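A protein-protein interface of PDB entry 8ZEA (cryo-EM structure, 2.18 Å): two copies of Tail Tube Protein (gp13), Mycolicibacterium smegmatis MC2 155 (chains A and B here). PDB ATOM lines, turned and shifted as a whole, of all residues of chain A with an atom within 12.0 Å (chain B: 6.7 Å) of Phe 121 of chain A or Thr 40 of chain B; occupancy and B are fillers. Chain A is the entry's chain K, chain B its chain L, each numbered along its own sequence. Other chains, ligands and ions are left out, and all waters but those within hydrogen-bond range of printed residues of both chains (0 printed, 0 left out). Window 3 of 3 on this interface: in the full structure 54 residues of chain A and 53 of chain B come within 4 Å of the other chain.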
ATOM      1  N   ILE A 116      -0.007 -17.450   8.655  1.00  0.00           N
ATOM      2  CA  ILE A 116       1.404 -17.370   9.007  1.00  0.00           C
ATOM      3  C   ILE A 116       1.879 -15.931   8.864  1.00  0.00           C
ATOM      4  O   ILE A 116       1.761 -15.322   7.793  1.00  0.00           O
ATOM      5  CB  ILE A 116       2.235 -18.320   8.130  1.00  0.00           C
ATOM      6  CG1 ILE A 116       1.990 -19.776   8.528  1.00  0.00           C
ATOM      7  CG2 ILE A 116       3.713 -17.981   8.231  1.00  0.00           C
ATOM      8  CD1 ILE A 116       2.171 -20.048  10.001  1.00  0.00           C
ATOM      9  N   GLN A 117       2.419 -15.382   9.943  1.00  0.00           N
ATOM     10  CA  GLN A 117       2.922 -14.021   9.950  1.00  0.00           C
ATOM     11  C   GLN A 117       4.439 -14.029   9.954  1.00  0.00           C
ATOM     12  O   GLN A 117       5.044 -14.691  10.808  1.00  0.00           O
ATOM     13  CB  GLN A 117       2.402 -13.257  11.172  1.00  0.00           C
ATOM     14  CG  GLN A 117       0.924 -12.915  11.104  1.00  0.00           C
ATOM     15  CD  GLN A 117       0.592 -12.012   9.937  1.00  0.00           C
ATOM     16  OE1 GLN A 117      -0.092 -12.419   8.996  1.00  0.00           O
ATOM     17  NE2 GLN A 117       1.079 -10.779   9.987  1.00  0.00           N
ATOM     18  N   PRO A 118       5.085 -13.335   9.022  1.00  0.00           N
ATOM     19  CA  PRO A 118       6.547 -13.249   9.054  1.00  0.00           C
ATOM     20  C   PRO A 118       7.022 -12.561  10.324  1.00  0.00           C
ATOM     21  O   PRO A 118       6.348 -11.691  10.878  1.00  0.00           O
ATOM     22  CB  PRO A 118       6.887 -12.423   7.807  1.00  0.00           C
ATOM     23  CG  PRO A 118       5.670 -12.502   6.946  1.00  0.00           C
ATOM     24  CD  PRO A 118       4.511 -12.616   7.874  1.00  0.00           C
ATOM     25  N   SER A 119       8.199 -12.969  10.786  1.00  0.00           N
ATOM     26  CA  SER A 119       8.764 -12.416  12.006  1.00  0.00           C
ATOM     27  C   SER A 119       9.249 -10.989  11.761  1.00  0.00           C
ATOM     28  O   SER A 119       9.065 -10.411  10.686  1.00  0.00           O
ATOM     29  CB  SER A 119       9.895 -13.307  12.513  1.00  0.00           C
ATOM     30  OG  SER A 119      11.071 -13.110  11.753  1.00  0.00           O
ATOM     31  N   GLU A 120       9.881 -10.413  12.787  1.00  0.00           N
ATOM     32  CA  GLU A 120      10.363  -9.038  12.692  1.00  0.00           C
ATOM     33  C   GLU A 120      11.322  -8.861  11.522  1.00  0.00           C
ATOM     34  O   GLU A 120      11.313  -7.824  10.850  1.00  0.00           O
ATOM     35  CB  GLU A 120      11.045  -8.632  14.001  1.00  0.00           C
ATOM     36  CG  GLU A 120      11.528  -7.195  14.019  1.00  0.00           C
ATOM     37  CD  GLU A 120      12.240  -6.828  15.304  1.00  0.00           C
ATOM     38  OE1 GLU A 120      12.361  -7.700  16.191  1.00  0.00           O
ATOM     39  OE2 GLU A 120      12.680  -5.666  15.426  1.00  0.00           O
ATOM     40  N   PHE A 121      12.148  -9.866  11.258  1.00  0.00           N
ATOM     41  CA  PHE A 121      13.123  -9.807  10.181  1.00  0.00           C
ATOM     42  C   PHE A 121      12.672 -10.570   8.943  1.00  0.00           C
ATOM     43  O   PHE A 121      13.488 -10.827   8.055  1.00  0.00           O
ATOM     44  CB  PHE A 121      14.470 -10.321  10.681  1.00  0.00           C
ATOM     45  CG  PHE A 121      14.959  -9.604  11.901  1.00  0.00           C
ATOM     46  CD1 PHE A 121      15.649  -8.411  11.788  1.00  0.00           C
ATOM     47  CD2 PHE A 121      14.703 -10.106  13.164  1.00  0.00           C
ATOM     48  CE1 PHE A 121      16.088  -7.742  12.910  1.00  0.00           C
ATOM     49  CE2 PHE A 121      15.141  -9.442  14.286  1.00  0.00           C
ATOM     50  CZ  PHE A 121      15.832  -8.259  14.159  1.00  0.00           C
ATOM     51  N   GLY A 122      11.391 -10.924   8.861  1.00  0.00           N
ATOM     52  CA  GLY A 122      10.825 -11.543   7.684  1.00  0.00           C
ATOM     53  C   GLY A 122      10.810 -13.054   7.677  1.00  0.00           C
ATOM     54  O   GLY A 122      10.238 -13.641   6.752  1.00  0.00           O
ATOM     55  N   GLY A 123      11.407 -13.703   8.670  1.00  0.00           N
ATOM     56  CA  GLY A 123      11.463 -15.150   8.671  1.00  0.00           C
ATOM     57  C   GLY A 123      10.112 -15.783   8.939  1.00  0.00           C
ATOM     58  O   GLY A 123       9.260 -15.231   9.633  1.00  0.00           O
ATOM     59  N   ILE A 124       9.916 -16.967   8.371  1.00  0.00           N
ATOM     60  CA  ILE A 124       8.693 -17.732   8.567  1.00  0.00           C
ATOM     61  C   ILE A 124       9.057 -19.158   8.944  1.00  0.00           C
ATOM     62  O   ILE A 124      10.104 -19.679   8.550  1.00  0.00           O
ATOM     63  CB  ILE A 124       7.781 -17.722   7.316  1.00  0.00           C
ATOM     64  CG1 ILE A 124       8.524 -18.283   6.102  1.00  0.00           C
ATOM     65  CG2 ILE A 124       7.248 -16.324   7.040  1.00  0.00           C
ATOM     66  CD1 ILE A 124       7.612 -18.827   5.033  1.00  0.00           C
ATOM     67  N   VAL A 125       8.183 -19.784   9.722  1.00  0.00           N
ATOM     68  CA  VAL A 125       8.292 -21.195  10.066  1.00  0.00           C
ATOM     69  C   VAL A 125       6.957 -21.853   9.755  1.00  0.00           C
ATOM     70  O   VAL A 125       5.915 -21.419  10.258  1.00  0.00           O
ATOM     71  CB  VAL A 125       8.673 -21.401  11.546  1.00  0.00           C
ATOM     72  CG1 VAL A 125       8.683 -22.882  11.891  1.00  0.00           C
ATOM     73  CG2 VAL A 125      10.028 -20.786  11.837  1.00  0.00           C
ATOM     74  N   GLU B  37      16.116 -17.915  13.457  1.00  0.00           N
ATOM     75  CA  GLU B  37      16.337 -16.487  13.277  1.00  0.00           C
ATOM     76  C   GLU B  37      16.554 -15.839  14.640  1.00  0.00           C
ATOM     77  O   GLU B  37      15.705 -15.954  15.529  1.00  0.00           O
ATOM     78  CB  GLU B  37      15.150 -15.851  12.553  1.00  0.00           C
ATOM     79  CG  GLU B  37      15.362 -14.402  12.150  1.00  0.00           C
ATOM     80  CD  GLU B  37      14.395 -13.939  11.072  1.00  0.00           C
ATOM     81  OE1 GLU B  37      13.207 -13.730  11.388  1.00  0.00           O
ATOM     82  OE2 GLU B  37      14.824 -13.780   9.909  1.00  0.00           O
ATOM     83  N   SER B  38      17.689 -15.175  14.803  1.00  0.00           N
ATOM     84  CA  SER B  38      17.980 -14.497  16.060  1.00  0.00           C
ATOM     85  C   SER B  38      17.009 -13.339  16.264  1.00  0.00           C
ATOM     86  O   SER B  38      16.755 -12.576  15.326  1.00  0.00           O
ATOM     87  CB  SER B  38      19.417 -13.986  16.073  1.00  0.00           C
ATOM     88  OG  SER B  38      19.653 -13.154  17.191  1.00  0.00           O
ATOM     89  N   PRO B  39      16.444 -13.174  17.464  1.00  0.00           N
ATOM     90  CA  PRO B  39      15.513 -12.058  17.695  1.00  0.00           C
ATOM     91  C   PRO B  39      16.184 -10.695  17.711  1.00  0.00           C
ATOM     92  O   PRO B  39      15.480  -9.682  17.631  1.00  0.00           O
ATOM     93  CB  PRO B  39      14.901 -12.384  19.066  1.00  0.00           C
ATOM     94  CG  PRO B  39      15.291 -13.806  19.359  1.00  0.00           C
ATOM     95  CD  PRO B  39      16.585 -14.028  18.653  1.00  0.00           C
ATOM     96  N   THR B  40      17.512 -10.636  17.805  1.00  0.00           N
ATOM     97  CA  THR B  40      18.203  -9.358  17.925  1.00  0.00           C
ATOM     98  C   THR B  40      18.400  -8.698  16.565  1.00  0.00           C
ATOM     99  O   THR B  40      17.990  -7.552  16.354  1.00  0.00           O
ATOM    100  CB  THR B  40      19.552  -9.557  18.623  1.00  0.00           C
ATOM    101  OG1 THR B  40      19.339 -10.136  19.916  1.00  0.00           O
ATOM    102  CG2 THR B  40      20.269  -8.226  18.784  1.00  0.00           C
ATOM    103  N   ASP B  41      19.034  -9.405  15.632  1.00  0.00           N
ATOM    104  CA  ASP B  41      19.322  -8.851  14.318  1.00  0.00           C
ATOM    105  C   ASP B  41      18.861  -9.732  13.166  1.00  0.00           C
ATOM    106  O   ASP B  41      19.142  -9.402  12.010  1.00  0.00           O
ATOM    107  CB  ASP B  41      20.827  -8.578  14.169  1.00  0.00           C
ATOM    108  CG  ASP B  41      21.673  -9.813  14.408  1.00  0.00           C
ATOM    109  OD1 ASP B  41      21.120 -10.845  14.841  1.00  0.00           O
ATOM    110  OD2 ASP B  41      22.896  -9.753  14.163  1.00  0.00           O
ATOM    111  N   GLY B  42      18.169 -10.834  13.439  1.00  0.00           N
ATOM    112  CA  GLY B  42      17.719 -11.722  12.391  1.00  0.00           C
ATOM    113  C   GLY B  42      18.772 -12.655  11.842  1.00  0.00           C
ATOM    114  O   GLY B  42      18.481 -13.402  10.899  1.00  0.00           O
ATOM    115  N   SER B  43      19.981 -12.640  12.392  1.00  0.00           N
ATOM    116  CA  SER B  43      21.038 -13.515  11.915  1.00  0.00           C
ATOM    117  C   SER B  43      20.774 -14.958  12.337  1.00  0.00           C
ATOM    118  O   SER B  43      19.942 -15.244  13.199  1.00  0.00           O
ATOM    119  CB  SER B  43      22.395 -13.049  12.442  1.00  0.00           C
ATOM    120  OG  SER B  43      22.577 -13.436  13.791  1.00  0.00           O
ATOM    121  N   ALA B 200      14.647 -17.863   6.286  1.00  0.00           N
ATOM    122  CA  ALA B 200      15.169 -16.715   7.015  1.00  0.00           C
ATOM    123  C   ALA B 200      16.310 -16.097   6.217  1.00  0.00           C
ATOM    124  O   ALA B 200      16.750 -16.637   5.200  1.00  0.00           O
ATOM    125  CB  ALA B 200      15.623 -17.114   8.422  1.00  0.00           C
ATOM    126  N   GLY B 201      16.790 -14.950   6.691  1.00  0.00           N
ATOM    127  CA  GLY B 201      17.874 -14.249   6.050  1.00  0.00           C
ATOM    128  C   GLY B 201      17.428 -12.998   5.321  1.00  0.00           C
ATOM    129  O   GLY B 201      16.259 -12.845   4.959  1.00  0.00           O
ATOM    130  N   PRO B 202      18.359 -12.064   5.110  1.00  0.00           N
ATOM    131  CA  PRO B 202      18.015 -10.842   4.360  1.00  0.00           C
ATOM    132  C   PRO B 202      17.556 -11.118   2.939  1.00  0.00           C
ATOM    133  O   PRO B 202      16.645 -10.445   2.434  1.00  0.00           O
ATOM    134  CB  PRO B 202      19.321 -10.036   4.396  1.00  0.00           C
ATOM    135  CG  PRO B 202      20.388 -11.045   4.629  1.00  0.00           C
ATOM    136  CD  PRO B 202      19.782 -12.104   5.489  1.00  0.00           C
ATOM    137  N   TRP B 204      15.875 -13.720   2.032  1.00  0.00           N
ATOM    138  CA  TRP B 204      14.477 -14.104   2.180  1.00  0.00           C
ATOM    139  C   TRP B 204      13.602 -12.890   2.446  1.00  0.00           C
ATOM    140  O   TRP B 204      12.510 -12.774   1.880  1.00  0.00           O
ATOM    141  CB  TRP B 204      14.311 -15.125   3.301  1.00  0.00           C
ATOM    142  CG  TRP B 204      12.875 -15.429   3.581  1.00  0.00           C
ATOM    143  CD1 TRP B 204      12.163 -15.074   4.684  1.00  0.00           C
ATOM    144  CD2 TRP B 204      11.967 -16.131   2.725  1.00  0.00           C
ATOM    145  NE1 TRP B 204      10.872 -15.520   4.577  1.00  0.00           N
ATOM    146  CE2 TRP B 204      10.725 -16.174   3.382  1.00  0.00           C
ATOM    147  CE3 TRP B 204      12.088 -16.740   1.473  1.00  0.00           C
ATOM    148  CZ2 TRP B 204       9.609 -16.798   2.830  1.00  0.00           C
ATOM    149  CZ3 TRP B 204      10.980 -17.359   0.926  1.00  0.00           C
ATOM    150  CH2 TRP B 204       9.758 -17.383   1.605  1.00  0.00           C
ATOM    151  N   ARG B 205      14.071 -11.972   3.297  1.00  0.00           N
ATOM    152  CA  ARG B 205      13.304 -10.767   3.594  1.00  0.00           C
ATOM    153  C   ARG B 205      13.006  -9.969   2.335  1.00  0.00           C
ATOM    154  O   ARG B 205      11.957  -9.324   2.245  1.00  0.00           O
ATOM    155  CB  ARG B 205      14.052  -9.902   4.610  1.00  0.00           C
ATOM    156  CG  ARG B 205      13.296  -8.652   5.033  1.00  0.00           C
ATOM    157  CD  ARG B 205      13.934  -7.985   6.237  1.00  0.00           C
ATOM    158  NE  ARG B 205      15.328  -7.636   6.004  1.00  0.00           N
ATOM    159  CZ  ARG B 205      16.350  -8.153   6.670  1.00  0.00           C
ATOM    160  NH1 ARG B 205      16.171  -9.051   7.624  1.00  0.00           N
ATOM    161  NH2 ARG B 205      17.583  -7.760   6.371  1.00  0.00           N
ATOM    162  N   VAL B 208       9.744 -12.110   0.961  1.00  0.00           N
ATOM    163  CA  VAL B 208       8.652 -12.667   1.760  1.00  0.00           C
ATOM    164  C   VAL B 208       7.301 -12.271   1.178  1.00  0.00           C
ATOM    165  O   VAL B 208       6.389 -13.099   1.069  1.00  0.00           O
ATOM    166  CB  VAL B 208       8.763 -12.230   3.233  1.00  0.00           C
ATOM    167  CG1 VAL B 208       7.777 -13.010   4.081  1.00  0.00           C
ATOM    168  CG2 VAL B 208      10.149 -12.408   3.749  1.00  0.00           C
ATOM    169  N   GLY B 248       4.907  -4.936   9.060  1.00  0.00           N
ATOM    170  CA  GLY B 248       5.480  -5.261  10.348  1.00  0.00           C
ATOM    171  C   GLY B 248       6.884  -5.815  10.308  1.00  0.00           C
ATOM    172  O   GLY B 248       7.360  -6.322  11.329  1.00  0.00           O
ATOM    173  N   ILE B 249       7.563  -5.729   9.169  1.00  0.00           N
ATOM    174  CA  ILE B 249       8.905  -6.273   9.004  1.00  0.00           C
ATOM    175  C   ILE B 249       9.916  -5.156   9.217  1.00  0.00           C
ATOM    176  O   ILE B 249       9.780  -4.065   8.651  1.00  0.00           O
ATOM    177  CB  ILE B 249       9.077  -6.918   7.617  1.00  0.00           C
ATOM    178  CG1 ILE B 249       8.237  -8.190   7.516  1.00  0.00           C
ATOM    179  CG2 ILE B 249      10.536  -7.229   7.345  1.00  0.00           C
ATOM    180  CD1 ILE B 249       8.142  -8.746   6.124  1.00  0.00           C
ATOM    181  N   ASN B 250      10.920  -5.422  10.045  1.00  0.00           N
ATOM    182  CA  ASN B 250      11.998  -4.470  10.273  1.00  0.00           C
ATOM    183  C   ASN B 250      12.899  -4.409   9.045  1.00  0.00           C
ATOM    184  O   ASN B 250      13.575  -5.387   8.712  1.00  0.00           O
ATOM    185  CB  ASN B 250      12.792  -4.881  11.510  1.00  0.00           C
ATOM    186  CG  ASN B 250      13.775  -3.819  11.958  1.00  0.00           C
ATOM    187  OD1 ASN B 250      13.958  -2.801  11.296  1.00  0.00           O
ATOM    188  ND2 ASN B 250      14.417  -4.058  13.092  1.00  0.00           N
ATOM    189  N   PRO B 253      18.123  -2.965   8.249  1.00  0.00           N
ATOM    190  CA  PRO B 253      19.332  -3.338   7.497  1.00  0.00           C
ATOM    191  C   PRO B 253      19.239  -3.043   6.010  1.00  0.00           C
ATOM    192  O   PRO B 253      20.276  -2.956   5.343  1.00  0.00           O
ATOM    193  CB  PRO B 253      19.462  -4.844   7.765  1.00  0.00           C
ATOM    194  CG  PRO B 253      18.657  -5.093   8.985  1.00  0.00           C
ATOM    195  CD  PRO B 253      17.516  -4.141   8.898  1.00  0.00           C
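Of the 17 printed residues of chain B, 11 touch a printed residue of chain A.
Printed residues of chain B that touch a printed residue of chain A: Glu 37, Ser 38, Pro 39, Thr 40, Asp 41, Gly 42, Trp 204, Arg 205, Val 208, Ile 249 and Asn 250.
Hydrophobic or aromatic side chains of chain A that line the printed part of chain B: Pro 118, Phe 121 and Ile 124.
Among the printed residues, no Asp or Glu carboxylate lies within 4 Å of a Lys or Arg side-chain nitrogen of the other chain.
No position is printed for both chains.
Of the 17 pairs that touch across the chains among the printed residues, none has its exchanged pair printed and touching as well.
Of chain A, only Phe 121 comes within 4 Å of Thr 40 of chain B.
Of chain A, only Phe 121 comes within 4 Å of Ser 38 of chain B.
Of chain A, only Glu 120 (3.97 Å) and Phe 121 (3.4 Å) come within 4 Å of Pro 39 of chain B.
Of chain A, only Phe 121 (3.4 Å) comes within 4 Å of Asp 41 of chain B.
No residue of chain A comes within 4 Å of Ser 43 of chain B.
No residue of chain A comes within 4 Å of Ala 200 of chain B.
Gly 201 of chain B touches none of the printed residues of chain A.
No residue of chain A comes within 4 Å of Pro 202 of chain B.
Ile 249 of chain B touches two residues of chain A.
Asn 250 of chain B touches one residue of chain A.
Printed residues of chain B within 4 Å of Ser 119 of chain A: Glu 37 (2.3 Å) and Ile 249 (3.96 Å).
Printed residues of chain B within 4 Å of Glu 120 of chain A: Pro 39 (3.97 Å), Ile 249 (3.4 Å) and Asn 250 (2.6 Å).
Printed residues of chain B within 4 Å of Gly 122 of chain A: Trp 204 and Val 208.
Gln 117 of chain A touches none of the printed residues of chain B.
Ile 116 of chain A touches none of the printed residues of chain B.
The nearest residue of chain B that does not touch Phe 121 of chain A is Asn 250 of chain B (4.05 Å).
The nearest printed residue of chain B that does not touch Ser 119 of chain A is Gly 248 of chain B (4.5 Å).
Among the printed residues, pairs that only touch across the chains: Pro 118 of chain A with Val 208 of chain B, Ser 119 of chain A with Ile 249 of chain B, Glu 120 of chain A with Pro 39 of chain B, Glu 120 of chain A with Ile 249 of chain B, Phe 121 of chain A with Glu 37 of chain B, Phe 121 of chain A with Ser 38 of chain B, Phe 121 of chain A with Pro 39 of chain B, Phe 121 of chain A with Thr 40 of chain B, Phe 121 of chain A with Asp 41 of chain B, Phe 121 of chain A with Gly 42 of chain B, Gly 122 of chain A with Val 208 of chain B and Ile 124 of chain A with Trp 204 of chain B.
The side-chain hydroxyl (OG) of Ser 119 of chain A sits at hydrogen-bond distance from the backbone NH (N) of Gly 123 of chain A (3.2 Å).
OG of Ser 38 of chain B sits close to N of Thr 40 of chain B, at 3.4 Å.
OD1 of Asp 41 of chain B is in hydrogen-bond range of OG of Ser 43 of chain B (3.2 Å).
The side-chain hydroxyl (OG) of Ser 119 of chain A sits close to the backbone NH (N) of Phe 121 of chain A, at 3.5 Å.
N of Ser 38 of chain B sits at hydrogen-bond distance from O of Ser 43 of chain B (2.8 Å).
O of Gly 122 of chain A lies within hydrogen-bond range of NE1 of Trp 204 of chain B (2.9 Å).
The backbone carbonyl oxygen (O) of Glu 120 of chain A lies within hydrogen-bond range of the backbone NH (N) of Asn 250 of chain B.
OG of Ser 119 of chain A lies close to OE1 of Glu 37 of chain B (2.3 Å).
The backbone NH of Gly 123 of chain A is in hydrogen-bond range of the side-chain carboxylate of Glu 37 of chain B (3.3 Å).
O of Phe 121 of chain A is in hydrogen-bond range of NH1 of Arg 205 of chain B (3.2 Å).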
